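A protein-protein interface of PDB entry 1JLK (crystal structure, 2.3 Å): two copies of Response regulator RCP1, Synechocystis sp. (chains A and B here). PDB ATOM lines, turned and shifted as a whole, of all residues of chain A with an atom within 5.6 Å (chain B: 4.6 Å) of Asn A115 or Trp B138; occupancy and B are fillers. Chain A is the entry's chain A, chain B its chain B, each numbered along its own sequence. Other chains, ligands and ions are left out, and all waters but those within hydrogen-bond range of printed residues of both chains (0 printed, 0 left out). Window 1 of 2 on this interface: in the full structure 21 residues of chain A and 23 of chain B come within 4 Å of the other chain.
The side-chain amide nitrogen of Asn B115 is in hydrogen-bond range of the backbone carbonyl oxygen of Asn A115 (2.6 Å).
Of the printed residues of chain B, Tyr A110 touches Val B142.
Printed residues of chain B within 4 Å of Asn A115: Asn B115 (2.6 Å) and Trp B138 (3.3 Å).
Of the printed residues of chain B, Cys A116 touches Phe B137, Trp B138 and Val B142.
Printed residues of chain B within 4 Å of Phe A137: Cys B116, Ile B134, Phe B137 and Trp B138.
Trp B138 touches three residues of chain A.
Leu B139 touches none of the printed residues of chain A.
The nearest residue of chain B that does not touch Asn A115 is Val B114 (4.05 Å).
Printed residues of chain A that touch a printed residue of chain B: Tyr A110, Val A114, Asn A115, Cys A116, Tyr A117, Phe A137 and Trp A138.
Among the printed residues, 15 pairs touch across the chains.
Among the printed residues, no Asp or Glu carboxylate lies within 4 Å of a Lys or Arg side-chain nitrogen of the other chain.
Among the printed residues, merely in contact across the chains: Tyr A110 with Val B142, Val A114 with Asn B115, Asn A115 with Trp B138, Cys A116 with Phe B137, Cys A116 with Trp B138, Cys A116 with Val B142, Tyr A117 with Val B142, Phe A137 with Cys B116, Phe A137 with Ile B134, Phe A137 with Phe B137, Phe A137 with Trp B138, Trp A138 with Asn B115, Trp A138 with Cys B116 and Trp A138 with Phe B137.
Val A114 touches Asn B115, but with the chains exchanged Asn A115 does not touch Val B114 (4.05 Å).
Asn A115 touches its own counterpart, Asn B115.
Cys A116 touches Trp B138, and with the chains exchanged Trp A138 touches Cys B116.
Phe A137 touches its own counterpart, Phe B137.
Of the 15 pairs that touch across the chains among the printed residues, 10 have their exchanged pair printed and touching as well.
The side-chain amino group of Lys A84 is in hydrogen-bond range of the side-chain amide oxygen of Asn A115 (2.8 Å).
The backbone NH (N) of Val A94 is in hydrogen-bond range of the side-chain amide oxygen (OD1) of Asn A115, at 2.9 Å.
OH of Tyr A110 sits at hydrogen-bond distance from N of Tyr A117 (3.0 Å).
N of Val B142 is in hydrogen-bond range of O of Phe B137.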
ATOM      1  N   LYS A  84     -21.648  22.781 -24.007  1.00  0.00           N
ATOM      2  CA  LYS A  84     -22.693  22.164 -23.203  1.00  0.00           C
ATOM      3  C   LYS A  84     -23.232  23.040 -22.087  1.00  0.00           C
ATOM      4  O   LYS A  84     -24.164  22.646 -21.384  1.00  0.00           O
ATOM      5  CB  LYS A  84     -22.202  20.831 -22.640  1.00  0.00           C
ATOM      6  CG  LYS A  84     -21.978  19.771 -23.710  1.00  0.00           C
ATOM      7  CD  LYS A  84     -23.278  19.429 -24.423  1.00  0.00           C
ATOM      8  CE  LYS A  84     -23.102  18.257 -25.389  1.00  0.00           C
ATOM      9  NZ  LYS A  84     -24.359  17.973 -26.141  1.00  0.00           N
ATOM     10  N   ARG A  91     -28.015  21.513 -26.689  1.00  0.00           N
ATOM     11  CA  ARG A  91     -28.639  20.334 -27.282  1.00  0.00           C
ATOM     12  C   ARG A  91     -27.938  19.706 -28.498  1.00  0.00           C
ATOM     13  O   ARG A  91     -28.147  18.530 -28.799  1.00  0.00           O
ATOM     14  CB  ARG A  91     -30.095  20.673 -27.639  1.00  0.00           C
ATOM     15  CG  ARG A  91     -30.223  21.710 -28.742  1.00  0.00           C
ATOM     16  CD  ARG A  91     -31.671  22.075 -29.048  1.00  0.00           C
ATOM     17  NE  ARG A  91     -32.329  22.795 -27.954  1.00  0.00           N
ATOM     18  CZ  ARG A  91     -33.434  23.531 -28.102  1.00  0.00           C
ATOM     19  NH1 ARG A  91     -34.006  23.646 -29.296  1.00  0.00           N
ATOM     20  NH2 ARG A  91     -33.964  24.159 -27.061  1.00  0.00           N
ATOM     21  N   ILE A  92     -27.118  20.474 -29.201  1.00  0.00           N
ATOM     22  CA  ILE A  92     -26.414  19.940 -30.368  1.00  0.00           C
ATOM     23  C   ILE A  92     -25.525  18.770 -29.950  1.00  0.00           C
ATOM     24  O   ILE A  92     -24.594  18.952 -29.174  1.00  0.00           O
ATOM     25  CB  ILE A  92     -25.504  21.008 -31.021  1.00  0.00           C
ATOM     26  CG1 ILE A  92     -26.318  22.250 -31.365  1.00  0.00           C
ATOM     27  CG2 ILE A  92     -24.863  20.449 -32.288  1.00  0.00           C
ATOM     28  CD1 ILE A  92     -25.468  23.389 -31.895  1.00  0.00           C
ATOM     29  N   PRO A  93     -25.798  17.552 -30.461  1.00  0.00           N
ATOM     30  CA  PRO A  93     -24.977  16.391 -30.097  1.00  0.00           C
ATOM     31  C   PRO A  93     -23.494  16.628 -30.400  1.00  0.00           C
ATOM     32  O   PRO A  93     -23.147  17.165 -31.454  1.00  0.00           O
ATOM     33  CB  PRO A  93     -25.553  15.274 -30.972  1.00  0.00           C
ATOM     34  CG  PRO A  93     -26.987  15.667 -31.117  1.00  0.00           C
ATOM     35  CD  PRO A  93     -26.883  17.150 -31.378  1.00  0.00           C
ATOM     36  N   VAL A  94     -22.628  16.234 -29.474  1.00  0.00           N
ATOM     37  CA  VAL A  94     -21.192  16.380 -29.668  1.00  0.00           C
ATOM     38  C   VAL A  94     -20.534  15.026 -29.615  1.00  0.00           C
ATOM     39  O   VAL A  94     -20.637  14.315 -28.619  1.00  0.00           O
ATOM     40  CB  VAL A  94     -20.542  17.247 -28.593  1.00  0.00           C
ATOM     41  CG1 VAL A  94     -19.009  17.220 -28.772  1.00  0.00           C
ATOM     42  CG2 VAL A  94     -21.087  18.685 -28.685  1.00  0.00           C
ATOM     43  N   VAL A  95     -19.861  14.661 -30.694  1.00  0.00           N
ATOM     44  CA  VAL A  95     -19.193  13.376 -30.739  1.00  0.00           C
ATOM     45  C   VAL A  95     -17.701  13.581 -30.633  1.00  0.00           C
ATOM     46  O   VAL A  95     -17.061  14.015 -31.596  1.00  0.00           O
ATOM     47  CB  VAL A  95     -19.493  12.627 -32.044  1.00  0.00           C
ATOM     48  CG1 VAL A  95     -18.632  11.395 -32.132  1.00  0.00           C
ATOM     49  CG2 VAL A  95     -20.962  12.241 -32.092  1.00  0.00           C
ATOM     50  N   TYR A 110     -17.205  12.886 -20.311  1.00  0.00           N
ATOM     51  CA  TYR A 110     -18.554  12.475 -19.979  1.00  0.00           C
ATOM     52  C   TYR A 110     -19.135  13.379 -18.904  1.00  0.00           C
ATOM     53  O   TYR A 110     -20.294  13.771 -18.983  1.00  0.00           O
ATOM     54  CB  TYR A 110     -18.576  11.006 -19.541  1.00  0.00           C
ATOM     55  CG  TYR A 110     -18.704  10.078 -20.727  1.00  0.00           C
ATOM     56  CD1 TYR A 110     -17.648   9.260 -21.126  1.00  0.00           C
ATOM     57  CD2 TYR A 110     -19.868  10.073 -21.500  1.00  0.00           C
ATOM     58  CE1 TYR A 110     -17.747   8.467 -22.271  1.00  0.00           C
ATOM     59  CE2 TYR A 110     -19.978   9.281 -22.645  1.00  0.00           C
ATOM     60  CZ  TYR A 110     -18.916   8.484 -23.025  1.00  0.00           C
ATOM     61  OH  TYR A 110     -19.027   7.713 -24.167  1.00  0.00           O
ATOM     62  N   HIS A 113     -20.663  16.354 -20.135  1.00  0.00           N
ATOM     63  CA  HIS A 113     -21.842  16.130 -20.971  1.00  0.00           C
ATOM     64  C   HIS A 113     -21.626  15.845 -22.451  1.00  0.00           C
ATOM     65  O   HIS A 113     -22.436  16.249 -23.279  1.00  0.00           O
ATOM     66  CB  HIS A 113     -22.818  17.303 -20.834  1.00  0.00           C
ATOM     67  CG  HIS A 113     -23.340  17.486 -19.442  1.00  0.00           C
ATOM     68  ND1 HIS A 113     -22.881  18.476 -18.599  1.00  0.00           N
ATOM     69  CD2 HIS A 113     -24.254  16.780 -18.734  1.00  0.00           C
ATOM     70  CE1 HIS A 113     -23.490  18.371 -17.432  1.00  0.00           C
ATOM     71  NE2 HIS A 113     -24.328  17.350 -17.487  1.00  0.00           N
ATOM     72  N   VAL A 114     -20.548  15.151 -22.790  1.00  0.00           N
ATOM     73  CA  VAL A 114     -20.310  14.805 -24.184  1.00  0.00           C
ATOM     74  C   VAL A 114     -21.345  13.701 -24.464  1.00  0.00           C
ATOM     75  O   VAL A 114     -21.693  12.931 -23.560  1.00  0.00           O
ATOM     76  CB  VAL A 114     -18.873  14.265 -24.401  1.00  0.00           C
ATOM     77  CG1 VAL A 114     -18.775  12.813 -23.949  1.00  0.00           C
ATOM     78  CG2 VAL A 114     -18.468  14.423 -25.868  1.00  0.00           C
ATOM     79  N   ASN A 115     -21.860  13.636 -25.689  1.00  0.00           N
ATOM     80  CA  ASN A 115     -22.868  12.630 -26.006  1.00  0.00           C
ATOM     81  C   ASN A 115     -22.236  11.248 -26.053  1.00  0.00           C
ATOM     82  O   ASN A 115     -22.789  10.289 -25.520  1.00  0.00           O
ATOM     83  CB  ASN A 115     -23.580  13.002 -27.306  1.00  0.00           C
ATOM     84  CG  ASN A 115     -24.342  14.315 -27.186  1.00  0.00           C
ATOM     85  OD1 ASN A 115     -23.751  15.357 -26.900  1.00  0.00           O
ATOM     86  ND2 ASN A 115     -25.653  14.271 -27.395  1.00  0.00           N
ATOM     87  N   CYS A 116     -21.070  11.147 -26.675  1.00  0.00           N
ATOM     88  CA  CYS A 116     -20.334   9.888 -26.704  1.00  0.00           C
ATOM     89  C   CYS A 116     -18.875  10.208 -26.957  1.00  0.00           C
ATOM     90  O   CYS A 116     -18.547  11.268 -27.503  1.00  0.00           O
ATOM     91  CB  CYS A 116     -20.864   8.920 -27.779  1.00  0.00           C
ATOM     92  SG  CYS A 116     -20.880   9.515 -29.468  1.00  0.00           S
ATOM     93  N   TYR A 117     -17.999   9.303 -26.540  1.00  0.00           N
ATOM     94  CA  TYR A 117     -16.565   9.483 -26.721  1.00  0.00           C
ATOM     95  C   TYR A 117     -16.052   8.360 -27.627  1.00  0.00           C
ATOM     96  O   TYR A 117     -16.348   7.186 -27.402  1.00  0.00           O
ATOM     97  CB  TYR A 117     -15.874   9.424 -25.358  1.00  0.00           C
ATOM     98  CG  TYR A 117     -14.389   9.700 -25.375  1.00  0.00           C
ATOM     99  CD1 TYR A 117     -13.882  10.886 -24.838  1.00  0.00           C
ATOM    100  CD2 TYR A 117     -13.485   8.767 -25.900  1.00  0.00           C
ATOM    101  CE1 TYR A 117     -12.517  11.139 -24.811  1.00  0.00           C
ATOM    102  CE2 TYR A 117     -12.113   9.011 -25.883  1.00  0.00           C
ATOM    103  CZ  TYR A 117     -11.639  10.201 -25.332  1.00  0.00           C
ATOM    104  OH  TYR A 117     -10.292  10.446 -25.275  1.00  0.00           O
ATOM    105  N   PHE A 137     -25.325   6.062 -37.684  1.00  0.00           N
ATOM    106  CA  PHE A 137     -26.097   6.266 -36.465  1.00  0.00           C
ATOM    107  C   PHE A 137     -26.650   7.679 -36.263  1.00  0.00           C
ATOM    108  O   PHE A 137     -27.864   7.863 -36.144  1.00  0.00           O
ATOM    109  CB  PHE A 137     -25.261   5.872 -35.241  1.00  0.00           C
ATOM    110  CG  PHE A 137     -26.065   5.721 -33.978  1.00  0.00           C
ATOM    111  CD1 PHE A 137     -27.053   4.741 -33.878  1.00  0.00           C
ATOM    112  CD2 PHE A 137     -25.834   6.552 -32.885  1.00  0.00           C
ATOM    113  CE1 PHE A 137     -27.801   4.585 -32.708  1.00  0.00           C
ATOM    114  CE2 PHE A 137     -26.577   6.406 -31.705  1.00  0.00           C
ATOM    115  CZ  PHE A 137     -27.563   5.418 -31.622  1.00  0.00           C
ATOM    116  N   TRP A 138     -25.766   8.675 -36.231  1.00  0.00           N
ATOM    117  CA  TRP A 138     -26.192  10.050 -35.990  1.00  0.00           C
ATOM    118  C   TRP A 138     -26.943  10.796 -37.083  1.00  0.00           C
ATOM    119  O   TRP A 138     -27.763  11.662 -36.778  1.00  0.00           O
ATOM    120  CB  TRP A 138     -24.997  10.900 -35.538  1.00  0.00           C
ATOM    121  CG  TRP A 138     -24.466  10.437 -34.226  1.00  0.00           C
ATOM    122  CD1 TRP A 138     -23.425   9.579 -34.018  1.00  0.00           C
ATOM    123  CD2 TRP A 138     -24.999  10.745 -32.935  1.00  0.00           C
ATOM    124  NE1 TRP A 138     -23.278   9.333 -32.673  1.00  0.00           N
ATOM    125  CE2 TRP A 138     -24.231  10.035 -31.986  1.00  0.00           C
ATOM    126  CE3 TRP A 138     -26.056  11.548 -32.490  1.00  0.00           C
ATOM    127  CZ2 TRP A 138     -24.485  10.103 -30.609  1.00  0.00           C
ATOM    128  CZ3 TRP A 138     -26.312  11.618 -31.119  1.00  0.00           C
ATOM    129  CH2 TRP A 138     -25.527  10.900 -30.195  1.00  0.00           C
ATOM    130  N   LEU B  64     -24.251   1.588 -19.787  1.00  0.00           N
ATOM    131  CA  LEU B  64     -25.107   2.119 -20.845  1.00  0.00           C
ATOM    132  C   LEU B  64     -26.553   1.820 -20.504  1.00  0.00           C
ATOM    133  O   LEU B  64     -26.888   0.694 -20.137  1.00  0.00           O
ATOM    134  CB  LEU B  64     -24.763   1.476 -22.188  1.00  0.00           C
ATOM    135  CG  LEU B  64     -25.722   1.758 -23.349  1.00  0.00           C
ATOM    136  CD1 LEU B  64     -25.609   3.202 -23.768  1.00  0.00           C
ATOM    137  CD2 LEU B  64     -25.399   0.841 -24.518  1.00  0.00           C
ATOM    138  N   PRO B  93     -23.987   7.048 -20.183  1.00  0.00           N
ATOM    139  CA  PRO B  93     -24.763   7.356 -21.382  1.00  0.00           C
ATOM    140  C   PRO B  93     -26.166   6.758 -21.341  1.00  0.00           C
ATOM    141  O   PRO B  93     -26.352   5.616 -20.955  1.00  0.00           O
ATOM    142  CB  PRO B  93     -23.896   6.796 -22.520  1.00  0.00           C
ATOM    143  CG  PRO B  93     -22.909   5.897 -21.853  1.00  0.00           C
ATOM    144  CD  PRO B  93     -22.648   6.552 -20.537  1.00  0.00           C
ATOM    145  N   VAL B  95     -29.619   6.127 -23.653  1.00  0.00           N
ATOM    146  CA  VAL B  95     -30.167   6.124 -25.001  1.00  0.00           C
ATOM    147  C   VAL B  95     -31.678   6.002 -24.935  1.00  0.00           C
ATOM    148  O   VAL B  95     -32.207   4.960 -24.552  1.00  0.00           O
ATOM    149  CB  VAL B  95     -29.657   4.949 -25.828  1.00  0.00           C
ATOM    150  CG1 VAL B  95     -30.382   4.917 -27.175  1.00  0.00           C
ATOM    151  CG2 VAL B  95     -28.161   5.064 -26.021  1.00  0.00           C
ATOM    152  N   VAL B 114     -29.893  13.994 -22.554  1.00  0.00           N
ATOM    153  CA  VAL B 114     -29.981  12.604 -22.982  1.00  0.00           C
ATOM    154  C   VAL B 114     -28.888  12.509 -24.070  1.00  0.00           C
ATOM    155  O   VAL B 114     -28.643  13.484 -24.783  1.00  0.00           O
ATOM    156  CB  VAL B 114     -31.398  12.287 -23.570  1.00  0.00           C
ATOM    157  CG1 VAL B 114     -31.536  12.847 -24.974  1.00  0.00           C
ATOM    158  CG2 VAL B 114     -31.656  10.805 -23.539  1.00  0.00           C
ATOM    159  N   ASN B 115     -28.210  11.370 -24.181  1.00  0.00           N
ATOM    160  CA  ASN B 115     -27.146  11.226 -25.175  1.00  0.00           C
ATOM    161  C   ASN B 115     -27.669  11.174 -26.609  1.00  0.00           C
ATOM    162  O   ASN B 115     -27.051  11.719 -27.526  1.00  0.00           O
ATOM    163  CB  ASN B 115     -26.294   9.994 -24.862  1.00  0.00           C
ATOM    164  CG  ASN B 115     -25.680  10.057 -23.466  1.00  0.00           C
ATOM    165  OD1 ASN B 115     -26.396  10.026 -22.467  1.00  0.00           O
ATOM    166  ND2 ASN B 115     -24.356  10.155 -23.395  1.00  0.00           N
ATOM    167  N   CYS B 116     -28.792  10.499 -26.810  1.00  0.00           N
ATOM    168  CA  CYS B 116     -29.410  10.444 -28.126  1.00  0.00           C
ATOM    169  C   CYS B 116     -30.835   9.964 -27.953  1.00  0.00           C
ATOM    170  O   CYS B 116     -31.164   9.267 -26.992  1.00  0.00           O
ATOM    171  CB  CYS B 116     -28.631   9.541 -29.089  1.00  0.00           C
ATOM    172  SG  CYS B 116     -28.612   7.817 -28.668  1.00  0.00           S
ATOM    173  N   ILE B 134     -27.873   0.603 -32.705  1.00  0.00           N
ATOM    174  CA  ILE B 134     -27.518   0.996 -31.349  1.00  0.00           C
ATOM    175  C   ILE B 134     -26.384   0.097 -30.878  1.00  0.00           C
ATOM    176  O   ILE B 134     -25.381   0.572 -30.357  1.00  0.00           O
ATOM    177  CB  ILE B 134     -28.696   0.823 -30.370  1.00  0.00           C
ATOM    178  CG1 ILE B 134     -29.903   1.636 -30.830  1.00  0.00           C
ATOM    179  CG2 ILE B 134     -28.288   1.289 -28.983  1.00  0.00           C
ATOM    180  CD1 ILE B 134     -31.126   1.388 -29.982  1.00  0.00           C
ATOM    181  N   GLU B 135     -26.546  -1.205 -31.087  1.00  0.00           N
ATOM    182  CA  GLU B 135     -25.556  -2.189 -30.664  1.00  0.00           C
ATOM    183  C   GLU B 135     -24.196  -1.997 -31.306  1.00  0.00           C
ATOM    184  O   GLU B 135     -23.172  -2.060 -30.634  1.00  0.00           O
ATOM    185  CB  GLU B 135     -26.056  -3.610 -30.960  1.00  0.00           C
ATOM    186  CG  GLU B 135     -25.141  -4.707 -30.446  1.00  0.00           C
ATOM    187  CD  GLU B 135     -24.106  -5.140 -31.467  1.00  0.00           C
ATOM    188  OE1 GLU B 135     -23.057  -5.682 -31.053  1.00  0.00           O
ATOM    189  OE2 GLU B 135     -24.346  -4.962 -32.680  1.00  0.00           O
ATOM    190  N   SER B 136     -24.190  -1.765 -32.611  1.00  0.00           N
ATOM    191  CA  SER B 136     -22.943  -1.597 -33.328  1.00  0.00           C
ATOM    192  C   SER B 136     -22.268  -0.280 -32.976  1.00  0.00           C
ATOM    193  O   SER B 136     -21.047  -0.167 -33.048  1.00  0.00           O
ATOM    194  CB  SER B 136     -23.183  -1.666 -34.839  1.00  0.00           C
ATOM    195  OG  SER B 136     -23.791  -0.478 -35.319  1.00  0.00           O
ATOM    196  N   PHE B 137     -23.045   0.721 -32.585  1.00  0.00           N
ATOM    197  CA  PHE B 137     -22.423   1.988 -32.254  1.00  0.00           C
ATOM    198  C   PHE B 137     -22.056   2.116 -30.775  1.00  0.00           C
ATOM    199  O   PHE B 137     -20.902   2.364 -30.425  1.00  0.00           O
ATOM    200  CB  PHE B 137     -23.319   3.149 -32.658  1.00  0.00           C
ATOM    201  CG  PHE B 137     -22.664   4.484 -32.485  1.00  0.00           C
ATOM    202  CD1 PHE B 137     -21.631   4.874 -33.328  1.00  0.00           C
ATOM    203  CD2 PHE B 137     -23.043   5.331 -31.453  1.00  0.00           C
ATOM    204  CE1 PHE B 137     -20.978   6.091 -33.152  1.00  0.00           C
ATOM    205  CE2 PHE B 137     -22.393   6.558 -31.267  1.00  0.00           C
ATOM    206  CZ  PHE B 137     -21.358   6.933 -32.121  1.00  0.00           C
ATOM    207  N   TRP B 138     -23.030   1.939 -29.895  1.00  0.00           N
ATOM    208  CA  TRP B 138     -22.742   2.061 -28.481  1.00  0.00           C
ATOM    209  C   TRP B 138     -21.926   0.935 -27.862  1.00  0.00           C
ATOM    210  O   TRP B 138     -21.191   1.173 -26.909  1.00  0.00           O
ATOM    211  CB  TRP B 138     -24.035   2.267 -27.711  1.00  0.00           C
ATOM    212  CG  TRP B 138     -24.621   3.600 -28.009  1.00  0.00           C
ATOM    213  CD1 TRP B 138     -25.548   3.895 -28.960  1.00  0.00           C
ATOM    214  CD2 TRP B 138     -24.272   4.840 -27.387  1.00  0.00           C
ATOM    215  NE1 TRP B 138     -25.802   5.243 -28.974  1.00  0.00           N
ATOM    216  CE2 TRP B 138     -25.032   5.849 -28.016  1.00  0.00           C
ATOM    217  CE3 TRP B 138     -23.387   5.196 -26.357  1.00  0.00           C
ATOM    218  CZ2 TRP B 138     -24.940   7.194 -27.652  1.00  0.00           C
ATOM    219  CZ3 TRP B 138     -23.291   6.533 -25.995  1.00  0.00           C
ATOM    220  CH2 TRP B 138     -24.066   7.517 -26.641  1.00  0.00           C
ATOM    221  N   LEU B 139     -22.029  -0.280 -28.390  1.00  0.00           N
ATOM    222  CA  LEU B 139     -21.257  -1.385 -27.817  1.00  0.00           C
ATOM    223  C   LEU B 139     -19.942  -1.716 -28.512  1.00  0.00           C
ATOM    224  O   LEU B 139     -19.084  -2.379 -27.923  1.00  0.00           O
ATOM    225  CB  LEU B 139     -22.096  -2.661 -27.741  1.00  0.00           C
ATOM    226  CG  LEU B 139     -23.019  -2.780 -26.534  1.00  0.00           C
ATOM    227  CD1 LEU B 139     -24.268  -1.937 -26.767  1.00  0.00           C
ATOM    228  CD2 LEU B 139     -23.391  -4.244 -26.319  1.00  0.00           C
ATOM    229  N   GLU B 140     -19.775  -1.268 -29.754  1.00  0.00           N
ATOM    230  CA  GLU B 140     -18.544  -1.560 -30.486  1.00  0.00           C
ATOM    231  C   GLU B 140     -17.662  -0.356 -30.756  1.00  0.00           C
ATOM    232  O   GLU B 140     -16.460  -0.413 -30.531  1.00  0.00           O
ATOM    233  CB  GLU B 140     -18.854  -2.227 -31.831  1.00  0.00           C
ATOM    234  CG  GLU B 140     -19.817  -3.385 -31.739  1.00  0.00           C
ATOM    235  CD  GLU B 140     -19.904  -4.186 -33.027  1.00  0.00           C
ATOM    236  OE1 GLU B 140     -20.111  -3.580 -34.106  1.00  0.00           O
ATOM    237  OE2 GLU B 140     -19.776  -5.429 -32.953  1.00  0.00           O
ATOM    238  N   VAL B 142     -18.264   3.107 -29.637  1.00  0.00           N
ATOM    239  CA  VAL B 142     -18.185   4.011 -28.501  1.00  0.00           C
ATOM    240  C   VAL B 142     -17.392   3.484 -27.321  1.00  0.00           C
ATOM    241  O   VAL B 142     -17.523   2.325 -26.927  1.00  0.00           O
ATOM    242  CB  VAL B 142     -19.592   4.379 -27.996  1.00  0.00           C
ATOM    243  CG1 VAL B 142     -19.499   5.131 -26.680  1.00  0.00           C
ATOM    244  CG2 VAL B 142     -20.293   5.229 -29.026  1.00  0.00           C
ATOM    245  N   LEU B 144     -17.233   3.408 -23.718  1.00  0.00           N
ATOM    246  CA  LEU B 144     -18.083   3.677 -22.571  1.00  0.00           C
ATOM    247  C   LEU B 144     -17.268   4.112 -21.368  1.00  0.00           C
ATOM    248  O   LEU B 144     -16.140   3.669 -21.176  1.00  0.00           O
ATOM    249  CB  LEU B 144     -18.903   2.440 -22.221  1.00  0.00           C
ATOM    250  CG  LEU B 144     -19.894   2.046 -23.306  1.00  0.00           C
ATOM    251  CD1 LEU B 144     -20.567   0.735 -22.926  1.00  0.00           C
ATOM    252  CD2 LEU B 144     -20.920   3.166 -23.485  1.00  0.00           C
